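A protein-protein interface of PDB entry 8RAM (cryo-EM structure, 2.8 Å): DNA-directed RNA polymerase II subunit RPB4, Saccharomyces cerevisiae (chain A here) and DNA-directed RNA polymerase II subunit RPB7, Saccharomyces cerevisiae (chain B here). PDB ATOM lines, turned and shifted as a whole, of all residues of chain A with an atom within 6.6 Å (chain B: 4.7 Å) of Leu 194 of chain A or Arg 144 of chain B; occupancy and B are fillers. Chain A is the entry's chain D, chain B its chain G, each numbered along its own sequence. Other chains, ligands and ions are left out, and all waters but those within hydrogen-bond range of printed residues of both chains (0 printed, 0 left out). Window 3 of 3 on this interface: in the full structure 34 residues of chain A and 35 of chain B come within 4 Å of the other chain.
Hydrophobic or aromatic side chains of chain A within 4 Å of the printed part of chain B: Leu 183 and Leu 194. Hydrophobic or aromatic side chains of chain B that line the printed part of chain A: Val 86 and Tyr 167. Along chain B the printed residues that touch a printed residue of chain A span positions 86 to 167. Among the printed residues, 5 pairs touch across the chains. Among the printed residues, no Asp or Glu carboxylate lies within 4 Å of a Lys or Arg side-chain nitrogen of the other chain.
Among the printed residues, pairs that only touch across the chains: Leu 183 of chain A with Val 86 of chain B, Leu 183 of chain A with Arg 144 of chain B, Glu 190 of chain A with Tyr 167 of chain B, Leu 194 of chain A with Val 86 of chain B and Leu 194 of chain A with Arg 144 of chain B.
Of the printed residues of chain B, Glu 190 of chain A touches Tyr 167 (3.3 Å). Printed residues of chain B within 4 Å of Leu 194 of chain A: Val 86 and Arg 144. Printed residues of chain A within 4 Å of Val 86 of chain B: Leu 183 and Leu 194. Of the printed residues of chain A, Arg 144 of chain B touches Leu 183 and Leu 194. Of the printed residues of chain A, Tyr 167 of chain B touches Glu 190 (3.3 Å). Leu 168 of chain B touches none of the printed residues of chain A. Ile 171 of chain B touches none of the printed residues of chain A. The nearest printed residue of chain B that does not touch Leu 194 of chain A is Lys 146 of chain B (5.1 Å).
The backbone carbonyl oxygen of Arg 144 of chain B is in hydrogen-bond range of the backbone NH of Gly 169 of chain B (3.1 Å).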
ATOM      1  N   ALA A  25      -1.430   5.811 -21.495  1.00  0.00           N
ATOM      2  CA  ALA A  25      -2.380   5.438 -20.457  1.00  0.00           C
ATOM      3  C   ALA A  25      -2.737   6.598 -19.535  1.00  0.00           C
ATOM      4  O   ALA A  25      -3.451   6.390 -18.549  1.00  0.00           O
ATOM      5  CB  ALA A  25      -1.820   4.276 -19.630  1.00  0.00           C
ATOM      6  N   GLN A 179     -11.207  -2.122 -18.593  1.00  0.00           N
ATOM      7  CA  GLN A 179      -9.990  -2.812 -18.174  1.00  0.00           C
ATOM      8  C   GLN A 179     -10.202  -3.547 -16.858  1.00  0.00           C
ATOM      9  O   GLN A 179      -9.759  -4.691 -16.698  1.00  0.00           O
ATOM     10  CB  GLN A 179      -8.836  -1.817 -18.049  1.00  0.00           C
ATOM     11  CG  GLN A 179      -8.313  -1.303 -19.379  1.00  0.00           C
ATOM     12  CD  GLN A 179      -7.037  -0.495 -19.232  1.00  0.00           C
ATOM     13  OE1 GLN A 179      -6.130  -0.596 -20.057  1.00  0.00           O
ATOM     14  NE2 GLN A 179      -6.964   0.318 -18.183  1.00  0.00           N
ATOM     15  N   LEU A 180     -10.878  -2.908 -15.901  1.00  0.00           N
ATOM     16  CA  LEU A 180     -11.119  -3.554 -14.615  1.00  0.00           C
ATOM     17  C   LEU A 180     -11.961  -4.814 -14.782  1.00  0.00           C
ATOM     18  O   LEU A 180     -11.680  -5.845 -14.160  1.00  0.00           O
ATOM     19  CB  LEU A 180     -11.800  -2.578 -13.657  1.00  0.00           C
ATOM     20  CG  LEU A 180     -10.953  -1.395 -13.180  1.00  0.00           C
ATOM     21  CD1 LEU A 180     -11.801  -0.424 -12.374  1.00  0.00           C
ATOM     22  CD2 LEU A 180      -9.763  -1.873 -12.362  1.00  0.00           C
ATOM     23  N   LEU A 183      -9.320  -7.224 -17.315  1.00  0.00           N
ATOM     24  CA  LEU A 183      -8.092  -7.619 -16.641  1.00  0.00           C
ATOM     25  C   LEU A 183      -8.387  -8.051 -15.209  1.00  0.00           C
ATOM     26  O   LEU A 183      -9.286  -7.527 -14.547  1.00  0.00           O
ATOM     27  CB  LEU A 183      -7.082  -6.471 -16.647  1.00  0.00           C
ATOM     28  CG  LEU A 183      -6.403  -6.173 -17.989  1.00  0.00           C
ATOM     29  CD1 LEU A 183      -7.403  -5.673 -19.022  1.00  0.00           C
ATOM     30  CD2 LEU A 183      -5.276  -5.169 -17.807  1.00  0.00           C
ATOM     31  N   ALA A 184      -7.612  -9.021 -14.731  1.00  0.00           N
ATOM     32  CA  ALA A 184      -7.792  -9.595 -13.405  1.00  0.00           C
ATOM     33  C   ALA A 184      -6.708  -9.078 -12.468  1.00  0.00           C
ATOM     34  O   ALA A 184      -5.521  -9.097 -12.813  1.00  0.00           O
ATOM     35  CB  ALA A 184      -7.752 -11.123 -13.463  1.00  0.00           C
ATOM     36  N   CYS A 185      -7.120  -8.618 -11.289  1.00  0.00           N
ATOM     37  CA  CYS A 185      -6.206  -8.118 -10.274  1.00  0.00           C
ATOM     38  C   CYS A 185      -6.585  -8.703  -8.922  1.00  0.00           C
ATOM     39  O   CYS A 185      -7.746  -9.045  -8.678  1.00  0.00           O
ATOM     40  CB  CYS A 185      -6.228  -6.585 -10.204  1.00  0.00           C
ATOM     41  SG  CYS A 185      -5.750  -5.765 -11.744  1.00  0.00           S
ATOM     42  N   ASP A 189      -1.837  -2.779  -4.778  1.00  0.00           N
ATOM     43  CA  ASP A 189      -0.613  -2.295  -5.408  1.00  0.00           C
ATOM     44  C   ASP A 189      -0.534  -2.734  -6.864  1.00  0.00           C
ATOM     45  O   ASP A 189      -0.121  -1.957  -7.735  1.00  0.00           O
ATOM     46  CB  ASP A 189       0.607  -2.790  -4.631  1.00  0.00           C
ATOM     47  CG  ASP A 189       1.907  -2.203  -5.147  1.00  0.00           C
ATOM     48  OD1 ASP A 189       1.857  -1.330  -6.039  1.00  0.00           O
ATOM     49  OD2 ASP A 189       2.981  -2.614  -4.659  1.00  0.00           O
ATOM     50  N   GLU A 190      -0.917  -3.983  -7.147  1.00  0.00           N
ATOM     51  CA  GLU A 190      -0.890  -4.467  -8.523  1.00  0.00           C
ATOM     52  C   GLU A 190      -1.840  -3.665  -9.403  1.00  0.00           C
ATOM     53  O   GLU A 190      -1.494  -3.298 -10.532  1.00  0.00           O
ATOM     54  CB  GLU A 190      -1.248  -5.954  -8.561  1.00  0.00           C
ATOM     55  CG  GLU A 190      -1.178  -6.583  -9.946  1.00  0.00           C
ATOM     56  CD  GLU A 190       0.225  -6.579 -10.522  1.00  0.00           C
ATOM     57  OE1 GLU A 190       1.180  -6.295  -9.769  1.00  0.00           O
ATOM     58  OE2 GLU A 190       0.374  -6.862 -11.729  1.00  0.00           O
ATOM     59  N   ALA A 191      -3.045  -3.381  -8.903  1.00  0.00           N
ATOM     60  CA  ALA A 191      -3.990  -2.582  -9.676  1.00  0.00           C
ATOM     61  C   ALA A 191      -3.463  -1.171  -9.899  1.00  0.00           C
ATOM     62  O   ALA A 191      -3.581  -0.623 -11.003  1.00  0.00           O
ATOM     63  CB  ALA A 191      -5.343  -2.542  -8.965  1.00  0.00           C
ATOM     64  N   LYS A 192      -2.876  -0.564  -8.865  1.00  0.00           N
ATOM     65  CA  LYS A 192      -2.370   0.798  -9.000  1.00  0.00           C
ATOM     66  C   LYS A 192      -1.235   0.870 -10.013  1.00  0.00           C
ATOM     67  O   LYS A 192      -1.201   1.778 -10.853  1.00  0.00           O
ATOM     68  CB  LYS A 192      -1.908   1.323  -7.640  1.00  0.00           C
ATOM     69  CG  LYS A 192      -3.033   1.532  -6.635  1.00  0.00           C
ATOM     70  CD  LYS A 192      -3.953   2.673  -7.043  1.00  0.00           C
ATOM     71  CE  LYS A 192      -5.045   2.901  -6.012  1.00  0.00           C
ATOM     72  NZ  LYS A 192      -5.965   4.004  -6.405  1.00  0.00           N
ATOM     73  N   THR A 193      -0.295  -0.077  -9.955  1.00  0.00           N
ATOM     74  CA  THR A 193       0.809  -0.063 -10.911  1.00  0.00           C
ATOM     75  C   THR A 193       0.340  -0.441 -12.310  1.00  0.00           C
ATOM     76  O   THR A 193       0.949  -0.019 -13.300  1.00  0.00           O
ATOM     77  CB  THR A 193       1.926  -1.004 -10.453  1.00  0.00           C
ATOM     78  OG1 THR A 193       3.053  -0.873 -11.329  1.00  0.00           O
ATOM     79  CG2 THR A 193       1.457  -2.451 -10.455  1.00  0.00           C
ATOM     80  N   LEU A 194      -0.731  -1.230 -12.413  1.00  0.00           N
ATOM     81  CA  LEU A 194      -1.275  -1.569 -13.724  1.00  0.00           C
ATOM     82  C   LEU A 194      -1.772  -0.326 -14.449  1.00  0.00           C
ATOM     83  O   LEU A 194      -1.541  -0.164 -15.653  1.00  0.00           O
ATOM     84  CB  LEU A 194      -2.404  -2.588 -13.567  1.00  0.00           C
ATOM     85  CG  LEU A 194      -3.147  -2.994 -14.841  1.00  0.00           C
ATOM     86  CD1 LEU A 194      -2.190  -3.604 -15.851  1.00  0.00           C
ATOM     87  CD2 LEU A 194      -4.269  -3.965 -14.508  1.00  0.00           C
ATOM     88  N   ILE A 195      -2.457   0.562 -13.733  1.00  0.00           N
ATOM     89  CA  ILE A 195      -2.984   1.798 -14.307  1.00  0.00           C
ATOM     90  C   ILE A 195      -2.559   2.965 -13.422  1.00  0.00           C
ATOM     91  O   ILE A 195      -3.368   3.470 -12.631  1.00  0.00           O
ATOM     92  CB  ILE A 195      -4.512   1.735 -14.462  1.00  0.00           C
ATOM     93  CG1 ILE A 195      -5.161   1.155 -13.201  1.00  0.00           C
ATOM     94  CG2 ILE A 195      -4.884   0.905 -15.682  1.00  0.00           C
ATOM     95  CD1 ILE A 195      -6.673   1.102 -13.263  1.00  0.00           C
ATOM     96  N   PRO A 196      -1.309   3.426 -13.519  1.00  0.00           N
ATOM     97  CA  PRO A 196      -0.869   4.527 -12.647  1.00  0.00           C
ATOM     98  C   PRO A 196      -1.709   5.782 -12.786  1.00  0.00           C
ATOM     99  O   PRO A 196      -1.862   6.525 -11.808  1.00  0.00           O
ATOM    100  CB  PRO A 196       0.582   4.765 -13.091  1.00  0.00           C
ATOM    101  CG  PRO A 196       1.009   3.483 -13.723  1.00  0.00           C
ATOM    102  CD  PRO A 196      -0.218   2.922 -14.372  1.00  0.00           C
ATOM    103  N   SER A 197      -2.259   6.046 -13.974  1.00  0.00           N
ATOM    104  CA  SER A 197      -3.069   7.246 -14.159  1.00  0.00           C
ATOM    105  C   SER A 197      -4.287   7.234 -13.244  1.00  0.00           C
ATOM    106  O   SER A 197      -4.636   8.261 -12.650  1.00  0.00           O
ATOM    107  CB  SER A 197      -3.499   7.365 -15.621  1.00  0.00           C
ATOM    108  OG  SER A 197      -4.279   6.249 -16.014  1.00  0.00           O
ATOM    109  N   VAL B  86      -1.959  -3.698 -21.068  1.00  0.00           N
ATOM    110  CA  VAL B  86      -1.515  -5.064 -20.820  1.00  0.00           C
ATOM    111  C   VAL B  86      -2.560  -6.011 -21.391  1.00  0.00           C
ATOM    112  O   VAL B  86      -3.743  -5.921 -21.039  1.00  0.00           O
ATOM    113  CB  VAL B  86      -1.304  -5.326 -19.318  1.00  0.00           C
ATOM    114  CG1 VAL B  86      -0.457  -6.575 -19.110  1.00  0.00           C
ATOM    115  CG2 VAL B  86      -0.671  -4.113 -18.653  1.00  0.00           C
ATOM    116  N   VAL B  87      -2.124  -6.915 -22.270  1.00  0.00           N
ATOM    117  CA  VAL B  87      -3.025  -7.841 -22.944  1.00  0.00           C
ATOM    118  C   VAL B  87      -2.411  -9.234 -22.924  1.00  0.00           C
ATOM    119  O   VAL B  87      -1.198  -9.404 -22.783  1.00  0.00           O
ATOM    120  CB  VAL B  87      -3.325  -7.408 -24.398  1.00  0.00           C
ATOM    121  CG1 VAL B  87      -4.565  -8.120 -24.923  1.00  0.00           C
ATOM    122  CG2 VAL B  87      -3.496  -5.899 -24.481  1.00  0.00           C
ATOM    123  N   ASP B  88      -3.271 -10.238 -23.075  1.00  0.00           N
ATOM    124  CA  ASP B  88      -2.870 -11.636 -23.044  1.00  0.00           C
ATOM    125  C   ASP B  88      -3.047 -12.263 -24.420  1.00  0.00           C
ATOM    126  O   ASP B  88      -4.053 -12.028 -25.097  1.00  0.00           O
ATOM    127  CB  ASP B  88      -3.683 -12.414 -22.004  1.00  0.00           C
ATOM    128  CG  ASP B  88      -5.166 -12.432 -22.317  1.00  0.00           C
ATOM    129  OD1 ASP B  88      -5.575 -13.177 -23.233  1.00  0.00           O
ATOM    130  OD2 ASP B  88      -5.925 -11.701 -21.647  1.00  0.00           O
ATOM    131  N   ARG B 142      -0.681 -19.318 -22.612  1.00  0.00           N
ATOM    132  CA  ARG B 142      -1.322 -18.014 -22.484  1.00  0.00           C
ATOM    133  C   ARG B 142      -0.376 -17.093 -21.722  1.00  0.00           C
ATOM    134  O   ARG B 142      -0.089 -17.327 -20.543  1.00  0.00           O
ATOM    135  CB  ARG B 142      -2.665 -18.148 -21.768  1.00  0.00           C
ATOM    136  CG  ARG B 142      -3.376 -16.832 -21.483  1.00  0.00           C
ATOM    137  CD  ARG B 142      -3.716 -16.077 -22.758  1.00  0.00           C
ATOM    138  NE  ARG B 142      -4.528 -16.870 -23.675  1.00  0.00           N
ATOM    139  CZ  ARG B 142      -5.039 -16.406 -24.812  1.00  0.00           C
ATOM    140  NH1 ARG B 142      -4.826 -15.148 -25.176  1.00  0.00           N
ATOM    141  NH2 ARG B 142      -5.767 -17.198 -25.587  1.00  0.00           N
ATOM    142  N   ILE B 143       0.110 -16.049 -22.389  1.00  0.00           N
ATOM    143  CA  ILE B 143       1.099 -15.139 -21.822  1.00  0.00           C
ATOM    144  C   ILE B 143       0.510 -13.736 -21.804  1.00  0.00           C
ATOM    145  O   ILE B 143       0.017 -13.252 -22.829  1.00  0.00           O
ATOM    146  CB  ILE B 143       2.419 -15.167 -22.615  1.00  0.00           C
ATOM    147  CG1 ILE B 143       2.927 -16.606 -22.745  1.00  0.00           C
ATOM    148  CG2 ILE B 143       3.468 -14.293 -21.936  1.00  0.00           C
ATOM    149  CD1 ILE B 143       4.234 -16.731 -23.496  1.00  0.00           C
ATOM    150  N   ARG B 144       0.569 -13.088 -20.643  1.00  0.00           N
ATOM    151  CA  ARG B 144       0.086 -11.724 -20.470  1.00  0.00           C
ATOM    152  C   ARG B 144       1.281 -10.781 -20.454  1.00  0.00           C
ATOM    153  O   ARG B 144       2.166 -10.909 -19.601  1.00  0.00           O
ATOM    154  CB  ARG B 144      -0.724 -11.601 -19.179  1.00  0.00           C
ATOM    155  CG  ARG B 144      -1.197 -10.191 -18.863  1.00  0.00           C
ATOM    156  CD  ARG B 144      -2.135 -10.187 -17.665  1.00  0.00           C
ATOM    157  NE  ARG B 144      -2.473  -8.834 -17.231  1.00  0.00           N
ATOM    158  CZ  ARG B 144      -1.757  -8.118 -16.368  1.00  0.00           C
ATOM    159  NH1 ARG B 144      -0.647  -8.614 -15.835  1.00  0.00           N
ATOM    160  NH2 ARG B 144      -2.151  -6.897 -16.037  1.00  0.00           N
ATOM    161  N   VAL B 145       1.307  -9.837 -21.397  1.00  0.00           N
ATOM    162  CA  VAL B 145       2.431  -8.929 -21.563  1.00  0.00           C
ATOM    163  C   VAL B 145       1.913  -7.505 -21.716  1.00  0.00           C
ATOM    164  O   VAL B 145       0.777  -7.267 -22.135  1.00  0.00           O
ATOM    165  CB  VAL B 145       3.308  -9.310 -22.777  1.00  0.00           C
ATOM    166  CG1 VAL B 145       3.733 -10.768 -22.688  1.00  0.00           C
ATOM    167  CG2 VAL B 145       2.564  -9.044 -24.079  1.00  0.00           C
ATOM    168  N   LYS B 146       2.779  -6.553 -21.377  1.00  0.00           N
ATOM    169  CA  LYS B 146       2.481  -5.136 -21.521  1.00  0.00           C
ATOM    170  C   LYS B 146       2.943  -4.643 -22.885  1.00  0.00           C
ATOM    171  O   LYS B 146       4.030  -4.998 -23.352  1.00  0.00           O
ATOM    172  CB  LYS B 146       3.162  -4.325 -20.417  1.00  0.00           C
ATOM    173  CG  LYS B 146       2.846  -4.800 -19.009  1.00  0.00           C
ATOM    174  CD  LYS B 146       3.326  -3.801 -17.967  1.00  0.00           C
ATOM    175  CE  LYS B 146       2.834  -4.164 -16.576  1.00  0.00           C
ATOM    176  NZ  LYS B 146       3.283  -3.182 -15.550  1.00  0.00           N
ATOM    177  N   ILE B 163       8.197  -7.785 -20.675  1.00  0.00           N
ATOM    178  CA  ILE B 163       7.750  -8.451 -19.451  1.00  0.00           C
ATOM    179  C   ILE B 163       8.798  -8.154 -18.382  1.00  0.00           C
ATOM    180  O   ILE B 163       9.798  -8.869 -18.252  1.00  0.00           O
ATOM    181  CB  ILE B 163       7.553  -9.959 -19.636  1.00  0.00           C
ATOM    182  CG1 ILE B 163       8.681 -10.549 -20.488  1.00  0.00           C
ATOM    183  CG2 ILE B 163       6.201 -10.240 -20.275  1.00  0.00           C
ATOM    184  CD1 ILE B 163       8.652 -12.061 -20.579  1.00  0.00           C
ATOM    185  N   TYR B 167       3.829 -10.201 -11.909  1.00  0.00           N
ATOM    186  CA  TYR B 167       2.570 -10.810 -12.327  1.00  0.00           C
ATOM    187  C   TYR B 167       2.472 -10.973 -13.838  1.00  0.00           C
ATOM    188  O   TYR B 167       1.393 -11.296 -14.351  1.00  0.00           O
ATOM    189  CB  TYR B 167       1.366 -10.005 -11.819  1.00  0.00           C
ATOM    190  CG  TYR B 167       0.061 -10.770 -11.824  1.00  0.00           C
ATOM    191  CD1 TYR B 167      -0.200 -11.742 -10.868  1.00  0.00           C
ATOM    192  CD2 TYR B 167      -0.915 -10.512 -12.778  1.00  0.00           C
ATOM    193  CE1 TYR B 167      -1.392 -12.442 -10.866  1.00  0.00           C
ATOM    194  CE2 TYR B 167      -2.109 -11.207 -12.785  1.00  0.00           C
ATOM    195  CZ  TYR B 167      -2.343 -12.169 -11.825  1.00  0.00           C
ATOM    196  OH  TYR B 167      -3.531 -12.864 -11.827  1.00  0.00           O
ATOM    197  N   LEU B 168       3.564 -10.769 -14.567  1.00  0.00           N
ATOM    198  CA  LEU B 168       3.582 -10.917 -16.014  1.00  0.00           C
ATOM    199  C   LEU B 168       4.088 -12.303 -16.400  1.00  0.00           C
ATOM    200  O   LEU B 168       4.632 -13.049 -15.582  1.00  0.00           O
ATOM    201  CB  LEU B 168       4.457  -9.834 -16.653  1.00  0.00           C
ATOM    202  CG  LEU B 168       4.018  -8.386 -16.427  1.00  0.00           C
ATOM    203  CD1 LEU B 168       5.025  -7.428 -17.042  1.00  0.00           C
ATOM    204  CD2 LEU B 168       2.629  -8.142 -16.997  1.00  0.00           C
ATOM    205  N   GLY B 169       3.897 -12.643 -17.672  1.00  0.00           N
ATOM    206  CA  GLY B 169       4.332 -13.926 -18.187  1.00  0.00           C
ATOM    207  C   GLY B 169       3.231 -14.967 -18.176  1.00  0.00           C
ATOM    208  O   GLY B 169       2.048 -14.631 -18.286  1.00  0.00           O
ATOM    209  N   ILE B 171       0.426 -17.461 -17.037  1.00  0.00           N
ATOM    210  CA  ILE B 171      -0.570 -17.371 -15.977  1.00  0.00           C
ATOM    211  C   ILE B 171      -1.464 -18.606 -15.998  1.00  0.00           C
ATOM    212  O   ILE B 171      -1.552 -19.307 -17.006  1.00  0.00           O
ATOM    213  CB  ILE B 171      -1.408 -16.086 -16.109  1.00  0.00           C
ATOM    214  CG1 ILE B 171      -2.070 -16.017 -17.489  1.00  0.00           C
ATOM    215  CG2 ILE B 171      -0.537 -14.862 -15.871  1.00  0.00           C
ATOM    216  CD1 ILE B 171      -2.961 -14.809 -17.682  1.00  0.00           C
ATOM    217  OXT ILE B 171      -2.119 -18.931 -15.008  1.00  0.00           O
